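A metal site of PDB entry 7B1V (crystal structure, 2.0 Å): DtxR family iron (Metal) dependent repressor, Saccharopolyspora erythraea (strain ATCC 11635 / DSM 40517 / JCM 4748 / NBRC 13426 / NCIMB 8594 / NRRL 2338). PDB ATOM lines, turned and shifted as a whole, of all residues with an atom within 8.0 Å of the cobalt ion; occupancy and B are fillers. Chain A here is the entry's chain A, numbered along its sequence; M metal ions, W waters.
The side-chain carboxylate of Glu 11 is in hydrogen-bond range of a ring nitrogen (ND1) of His 108 (2.7 Å). The side-chain carboxylate (OE1) of Glu 107 is in salt-bridge range of the guanidinium group (NH1) of Arg 15 (2.9 Å). The backbone carbonyl oxygen of Met 12 sits at hydrogen-bond distance from the side-chain hydroxyl of Thr 16 (2.6 Å). The side-chain carboxylate (OE1) of Glu 107 is in hydrogen-bond range of a ring nitrogen (ND1) of His 81. The backbone carbonyl oxygen of Leu 6 sits close to a ring nitrogen (NE2) of His 108, at 3.5 Å.
Four residues have an atom within 4 Å of the cobalt ion: Met 12, CSD 104, Glu 107 and His 108.
OE2 of Glu 107 is bound to the cobalt ion, 1.9 Å away. The cobalt ion is bound by O of CSD 104 (2.0 Å). The cobalt ion is bound by water W1. OD2 of CSD 104 is bound to the cobalt ion. NE2 of His 108 binds the cobalt ion (2.2 Å). The side-chain sulfur (SD) of Met 12 binds the cobalt ion, 2.5 Å away.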
ATOM      1  N   ASP A   5      33.935  -5.414  -9.762  1.00  0.00           N
ATOM      2  CA  ASP A   5      34.633  -5.419 -11.093  1.00  0.00           C
ATOM      3  C   ASP A   5      33.582  -5.223 -12.189  1.00  0.00           C
ATOM      4  O   ASP A   5      33.629  -4.170 -12.872  1.00  0.00           O
ATOM      5  CB  ASP A   5      35.442  -6.705 -11.274  1.00  0.00           C
ATOM      6  CG  ASP A   5      36.391  -6.678 -12.458  1.00  0.00           C
ATOM      7  OD1 ASP A   5      36.378  -5.675 -13.206  1.00  0.00           O
ATOM      8  OD2 ASP A   5      37.142  -7.667 -12.620  1.00  0.00           O
ATOM      9  N   LEU A   6      32.666  -6.176 -12.344  1.00  0.00           N
ATOM     10  CA  LEU A   6      31.493  -6.071 -13.260  1.00  0.00           C
ATOM     11  C   LEU A   6      30.470  -5.092 -12.681  1.00  0.00           C
ATOM     12  O   LEU A   6      29.556  -4.699 -13.428  1.00  0.00           O
ATOM     13  CB  LEU A   6      30.875  -7.463 -13.449  1.00  0.00           C
ATOM     14  CG  LEU A   6      31.757  -8.508 -14.131  1.00  0.00           C
ATOM     15  CD1 LEU A   6      31.133  -9.892 -14.032  1.00  0.00           C
ATOM     16  CD2 LEU A   6      32.016  -8.139 -15.585  1.00  0.00           C
ATOM     17  N   ILE A   7      30.625  -4.733 -11.395  1.00  0.00           N
ATOM     18  CA  ILE A   7      29.781  -3.763 -10.632  1.00  0.00           C
ATOM     19  C   ILE A   7      28.444  -4.423 -10.306  1.00  0.00           C
ATOM     20  O   ILE A   7      28.079  -4.446  -9.114  1.00  0.00           O
ATOM     21  CB  ILE A   7      29.603  -2.421 -11.387  1.00  0.00           C
ATOM     22  CG1 ILE A   7      30.941  -1.813 -11.815  1.00  0.00           C
ATOM     23  CG2 ILE A   7      28.785  -1.444 -10.554  1.00  0.00           C
ATOM     24  CD1 ILE A   7      31.881  -1.508 -10.675  1.00  0.00           C
ATOM     25  N   ASP A   8      27.730  -4.911 -11.324  1.00  0.00           N
ATOM     26  CA  ASP A   8      26.505  -5.731 -11.187  1.00  0.00           C
ATOM     27  C   ASP A   8      26.598  -6.912 -12.169  1.00  0.00           C
ATOM     28  O   ASP A   8      26.501  -6.671 -13.387  1.00  0.00           O
ATOM     29  CB  ASP A   8      25.246  -4.884 -11.405  1.00  0.00           C
ATOM     30  CG  ASP A   8      23.967  -5.530 -10.914  1.00  0.00           C
ATOM     31  OD1 ASP A   8      23.792  -6.748 -11.146  1.00  0.00           O
ATOM     32  OD2 ASP A   8      23.145  -4.817 -10.307  1.00  0.00           O
ATOM     33  N   THR A   9      26.796  -8.122 -11.649  1.00  0.00           N
ATOM     34  CA  THR A   9      27.004  -9.378 -12.423  1.00  0.00           C
ATOM     35  C   THR A   9      25.730  -9.718 -13.207  1.00  0.00           C
ATOM     36  O   THR A   9      25.854 -10.015 -14.407  1.00  0.00           O
ATOM     37  CB  THR A   9      27.413 -10.540 -11.498  1.00  0.00           C
ATOM     38  OG1 THR A   9      28.567 -10.127 -10.768  1.00  0.00           O
ATOM     39  CG2 THR A   9      27.720 -11.817 -12.249  1.00  0.00           C
ATOM     40  N   GLU A  11      23.138  -7.747 -14.188  1.00  0.00           N
ATOM     41  CA  GLU A  11      22.904  -6.729 -15.236  1.00  0.00           C
ATOM     42  C   GLU A  11      23.880  -6.932 -16.402  1.00  0.00           C
ATOM     43  O   GLU A  11      23.451  -6.746 -17.554  1.00  0.00           O
ATOM     44  CB  GLU A  11      23.029  -5.317 -14.652  1.00  0.00           C
ATOM     45  CG  GLU A  11      21.873  -4.935 -13.755  1.00  0.00           C
ATOM     46  CD  GLU A  11      21.905  -3.507 -13.236  1.00  0.00           C
ATOM     47  OE1 GLU A  11      22.985  -2.903 -13.233  1.00  0.00           O
ATOM     48  OE2 GLU A  11      20.836  -3.007 -12.827  1.00  0.00           O
ATOM     49  N   MET A  12      25.129  -7.314 -16.125  1.00  0.00           N
ATOM     50  CA  MET A  12      26.158  -7.561 -17.164  1.00  0.00           C
ATOM     51  C   MET A  12      25.859  -8.860 -17.912  1.00  0.00           C
ATOM     52  O   MET A  12      26.166  -8.919 -19.119  1.00  0.00           O
ATOM     53  CB  MET A  12      27.567  -7.609 -16.574  1.00  0.00           C
ATOM     54  CG  MET A  12      28.189  -6.236 -16.353  1.00  0.00           C
ATOM     55  SD  MET A  12      27.927  -5.116 -17.762  1.00  0.00           S
ATOM     56  CE  MET A  12      28.840  -5.977 -19.035  1.00  0.00           C
ATOM     57  N   TYR A  13      25.289  -9.863 -17.242  1.00  0.00           N
ATOM     58  CA  TYR A  13      24.801 -11.125 -17.864  1.00  0.00           C
ATOM     59  C   TYR A  13      23.602 -10.815 -18.750  1.00  0.00           C
ATOM     60  O   TYR A  13      23.519 -11.381 -19.859  1.00  0.00           O
ATOM     61  CB  TYR A  13      24.480 -12.182 -16.805  1.00  0.00           C
ATOM     62  CG  TYR A  13      25.651 -13.038 -16.389  1.00  0.00           C
ATOM     63  CD1 TYR A  13      26.807 -12.474 -15.873  1.00  0.00           C
ATOM     64  CD2 TYR A  13      25.601 -14.426 -16.487  1.00  0.00           C
ATOM     65  CE1 TYR A  13      27.884 -13.250 -15.495  1.00  0.00           C
ATOM     66  CE2 TYR A  13      26.679 -15.211 -16.105  1.00  0.00           C
ATOM     67  CZ  TYR A  13      27.820 -14.620 -15.603  1.00  0.00           C
ATOM     68  OH  TYR A  13      28.881 -15.383 -15.217  1.00  0.00           O
ATOM     69  N   ARG A  15      22.886  -7.804 -20.183  1.00  0.00           N
ATOM     70  CA  ARG A  15      23.290  -6.875 -21.270  1.00  0.00           C
ATOM     71  C   ARG A  15      24.144  -7.609 -22.303  1.00  0.00           C
ATOM     72  O   ARG A  15      24.050  -7.239 -23.495  1.00  0.00           O
ATOM     73  CB  ARG A  15      24.024  -5.655 -20.711  1.00  0.00           C
ATOM     74  CG  ARG A  15      23.825  -4.386 -21.540  1.00  0.00           C
ATOM     75  CD  ARG A  15      25.016  -3.459 -21.464  1.00  0.00           C
ATOM     76  NE  ARG A  15      26.120  -3.943 -22.290  1.00  0.00           N
ATOM     77  CZ  ARG A  15      27.355  -3.440 -22.276  1.00  0.00           C
ATOM     78  NH1 ARG A  15      27.659  -2.438 -21.463  1.00  0.00           N
ATOM     79  NH2 ARG A  15      28.284  -3.942 -23.060  1.00  0.00           N
ATOM     80  N   THR A  16      24.953  -8.591 -21.890  1.00  0.00           N
ATOM     81  CA  THR A  16      25.812  -9.404 -22.798  1.00  0.00           C
ATOM     82  C   THR A  16      24.931 -10.287 -23.691  1.00  0.00           C
ATOM     83  O   THR A  16      25.301 -10.473 -24.868  1.00  0.00           O
ATOM     84  CB  THR A  16      26.833 -10.251 -22.031  1.00  0.00           C
ATOM     85  OG1 THR A  16      26.186 -10.843 -20.899  1.00  0.00           O
ATOM     86  CG2 THR A  16      28.036  -9.441 -21.576  1.00  0.00           C
ATOM     87  N   LEU A  36      32.638 -12.059 -20.613  1.00  0.00           N
ATOM     88  CA  LEU A  36      32.791 -11.505 -19.244  1.00  0.00           C
ATOM     89  C   LEU A  36      33.988 -12.130 -18.524  1.00  0.00           C
ATOM     90  O   LEU A  36      34.213 -11.763 -17.353  1.00  0.00           O
ATOM     91  CB  LEU A  36      31.499 -11.763 -18.457  1.00  0.00           C
ATOM     92  CG  LEU A  36      30.248 -11.072 -19.011  1.00  0.00           C
ATOM     93  CD1 LEU A  36      29.028 -11.427 -18.175  1.00  0.00           C
ATOM     94  CD2 LEU A  36      30.437  -9.559 -19.065  1.00  0.00           C
ATOM     95  N   VAL A  77      19.493  -1.052 -18.728  1.00  0.00           N
ATOM     96  CA  VAL A  77      20.981  -1.030 -18.530  1.00  0.00           C
ATOM     97  C   VAL A  77      21.635  -0.431 -19.779  1.00  0.00           C
ATOM     98  O   VAL A  77      22.467   0.488 -19.623  1.00  0.00           O
ATOM     99  CB  VAL A  77      21.533  -2.441 -18.230  1.00  0.00           C
ATOM    100  CG1 VAL A  77      23.054  -2.479 -18.265  1.00  0.00           C
ATOM    101  CG2 VAL A  77      21.028  -2.967 -16.888  1.00  0.00           C
ATOM    102  N   HIS A  81      23.756   3.055 -20.218  1.00  0.00           N
ATOM    103  CA  HIS A  81      25.106   2.915 -20.845  1.00  0.00           C
ATOM    104  C   HIS A  81      25.276   3.960 -21.953  1.00  0.00           C
ATOM    105  O   HIS A  81      26.278   4.696 -21.913  1.00  0.00           O
ATOM    106  CB  HIS A  81      25.303   1.487 -21.376  1.00  0.00           C
ATOM    107  CG  HIS A  81      26.632   1.246 -22.011  1.00  0.00           C
ATOM    108  ND1 HIS A  81      27.734   0.849 -21.282  1.00  0.00           N
ATOM    109  CD2 HIS A  81      27.027   1.316 -23.303  1.00  0.00           C
ATOM    110  CE1 HIS A  81      28.758   0.701 -22.100  1.00  0.00           C
ATOM    111  NE2 HIS A  81      28.354   0.981 -23.341  1.00  0.00           N
ATOM    112  N   HIS A 100      33.577   3.989 -23.296  1.00  0.00           N
ATOM    113  CA  HIS A 100      32.807   2.717 -23.125  1.00  0.00           C
ATOM    114  C   HIS A 100      33.162   2.052 -21.792  1.00  0.00           C
ATOM    115  O   HIS A 100      32.234   1.574 -21.116  1.00  0.00           O
ATOM    116  CB  HIS A 100      33.043   1.747 -24.286  1.00  0.00           C
ATOM    117  CG  HIS A 100      32.526   0.377 -24.023  1.00  0.00           C
ATOM    118  ND1 HIS A 100      31.176   0.070 -24.132  1.00  0.00           N
ATOM    119  CD2 HIS A 100      33.142  -0.758 -23.632  1.00  0.00           C
ATOM    120  CE1 HIS A 100      30.996  -1.199 -23.821  1.00  0.00           C
ATOM    121  NE2 HIS A 100      32.187  -1.723 -23.519  1.00  0.00           N
ATOM    122  N   LEU A 101      34.452   2.007 -21.459  1.00  0.00           N
ATOM    123  CA  LEU A 101      34.977   1.399 -20.208  1.00  0.00           C
ATOM    124  C   LEU A 101      34.306   2.085 -19.006  1.00  0.00           C
ATOM    125  O   LEU A 101      33.905   1.368 -18.064  1.00  0.00           O
ATOM    126  CB  LEU A 101      36.502   1.540 -20.145  1.00  0.00           C
ATOM    127  CG  LEU A 101      37.300   0.462 -20.879  1.00  0.00           C
ATOM    128  CD1 LEU A 101      37.051   0.510 -22.381  1.00  0.00           C
ATOM    129  CD2 LEU A 101      38.783   0.596 -20.589  1.00  0.00           C
ATOM    130  N   GLU A 102      34.173   3.414 -19.073  1.00  0.00           N
ATOM    131  CA  GLU A 102      33.538   4.257 -18.020  1.00  0.00           C
ATOM    132  C   GLU A 102      32.039   3.948 -17.966  1.00  0.00           C
ATOM    133  O   GLU A 102      31.516   3.753 -16.844  1.00  0.00           O
ATOM    134  CB  GLU A 102      33.781   5.736 -18.322  1.00  0.00           C
ATOM    135  CG  GLU A 102      33.546   6.650 -17.138  1.00  0.00           C
ATOM    136  CD  GLU A 102      34.625   6.608 -16.061  1.00  0.00           C
ATOM    137  OE1 GLU A 102      35.761   6.220 -16.383  1.00  0.00           O
ATOM    138  OE2 GLU A 102      34.331   6.986 -14.919  1.00  0.00           O
ATOM    139  N   ALA A 103      31.377   3.889 -19.125  1.00  0.00           N
ATOM    140  CA  ALA A 103      29.929   3.635 -19.285  1.00  0.00           C
ATOM    141  C   ALA A 103      29.559   2.237 -18.805  1.00  0.00           C
ATOM    142  O   ALA A 103      28.429   1.995 -18.361  1.00  0.00           O
ATOM    143  CB  ALA A 103      29.534   3.843 -20.734  1.00  0.00           C
ATOM    144  N   CSD A 104      30.520   1.309 -18.906  1.00  0.00           N
ATOM    145  CA  CSD A 104      30.339  -0.070 -18.466  1.00  0.00           C
ATOM    146  CB  CSD A 104      31.532  -0.940 -18.864  1.00  0.00           C
ATOM    147  SG  CSD A 104      30.954  -2.466 -19.654  1.00  0.00           S
ATOM    148  C   CSD A 104      30.082  -0.138 -16.963  1.00  0.00           C
ATOM    149  O   CSD A 104      29.431  -1.061 -16.491  1.00  0.00           O
ATOM    150  OD1 CSD A 104      32.170  -3.121 -20.188  1.00  0.00           O
ATOM    151  OD2 CSD A 104      30.376  -3.400 -18.491  1.00  0.00           O
ATOM    152  N   ARG A 105      30.632   0.831 -16.215  1.00  0.00           N
ATOM    153  CA  ARG A 105      30.411   0.896 -14.783  1.00  0.00           C
ATOM    154  C   ARG A 105      29.218   1.807 -14.471  1.00  0.00           C
ATOM    155  O   ARG A 105      28.361   1.408 -13.655  1.00  0.00           O
ATOM    156  CB  ARG A 105      31.686   1.355 -14.077  1.00  0.00           C
ATOM    157  CG  ARG A 105      32.872   0.410 -14.261  1.00  0.00           C
ATOM    158  CD  ARG A 105      34.029   0.739 -13.336  1.00  0.00           C
ATOM    159  NE  ARG A 105      34.453   2.130 -13.491  1.00  0.00           N
ATOM    160  CZ  ARG A 105      35.206   2.598 -14.480  1.00  0.00           C
ATOM    161  NH1 ARG A 105      35.641   1.799 -15.442  1.00  0.00           N
ATOM    162  NH2 ARG A 105      35.508   3.882 -14.518  1.00  0.00           N
ATOM    163  N   TRP A 106      29.150   2.987 -15.099  1.00  0.00           N
ATOM    164  CA  TRP A 106      28.109   4.038 -14.875  1.00  0.00           C
ATOM    165  C   TRP A 106      26.704   3.467 -15.101  1.00  0.00           C
ATOM    166  O   TRP A 106      25.774   3.900 -14.383  1.00  0.00           O
ATOM    167  CB  TRP A 106      28.357   5.254 -15.777  1.00  0.00           C
ATOM    168  CG  TRP A 106      29.443   6.160 -15.293  1.00  0.00           C
ATOM    169  CD1 TRP A 106      30.615   5.800 -14.690  1.00  0.00           C
ATOM    170  CD2 TRP A 106      29.470   7.599 -15.388  1.00  0.00           C
ATOM    171  NE1 TRP A 106      31.360   6.914 -14.394  1.00  0.00           N
ATOM    172  CE2 TRP A 106      30.685   8.028 -14.809  1.00  0.00           C
ATOM    173  CE3 TRP A 106      28.583   8.551 -15.900  1.00  0.00           C
ATOM    174  CZ2 TRP A 106      31.027   9.376 -14.743  1.00  0.00           C
ATOM    175  CZ3 TRP A 106      28.932   9.884 -15.819  1.00  0.00           C
ATOM    176  CH2 TRP A 106      30.134  10.288 -15.248  1.00  0.00           C
ATOM    177  N   GLU A 107      26.541   2.557 -16.069  1.00  0.00           N
ATOM    178  CA  GLU A 107      25.240   1.959 -16.477  1.00  0.00           C
ATOM    179  C   GLU A 107      24.541   1.284 -15.281  1.00  0.00           C
ATOM    180  O   GLU A 107      23.309   1.181 -15.316  1.00  0.00           O
ATOM    181  CB  GLU A 107      25.440   0.962 -17.625  1.00  0.00           C
ATOM    182  CG  GLU A 107      26.328  -0.227 -17.271  1.00  0.00           C
ATOM    183  CD  GLU A 107      26.674  -1.133 -18.441  1.00  0.00           C
ATOM    184  OE1 GLU A 107      25.996  -1.039 -19.487  1.00  0.00           O
ATOM    185  OE2 GLU A 107      27.612  -1.933 -18.305  1.00  0.00           O
ATOM    186  N   HIS A 108      25.296   0.855 -14.267  1.00  0.00           N
ATOM    187  CA  HIS A 108      24.799   0.034 -13.121  1.00  0.00           C
ATOM    188  C   HIS A 108      24.366   0.912 -11.938  1.00  0.00           C
ATOM    189  O   HIS A 108      23.763   0.340 -10.999  1.00  0.00           O
ATOM    190  CB  HIS A 108      25.862  -0.993 -12.722  1.00  0.00           C
ATOM    191  CG  HIS A 108      26.295  -1.870 -13.852  1.00  0.00           C
ATOM    192  ND1 HIS A 108      25.431  -2.742 -14.478  1.00  0.00           N
ATOM    193  CD2 HIS A 108      27.484  -1.987 -14.466  1.00  0.00           C
ATOM    194  CE1 HIS A 108      26.076  -3.384 -15.432  1.00  0.00           C
ATOM    195  NE2 HIS A 108      27.340  -2.934 -15.447  1.00  0.00           N
HETATM  196 CO    CO M   1      28.803  -2.869 -17.123  1.00  0.00          CO
HETATM  197  O   HOH W   1      30.201  -3.502 -15.763  1.00  0.00           O
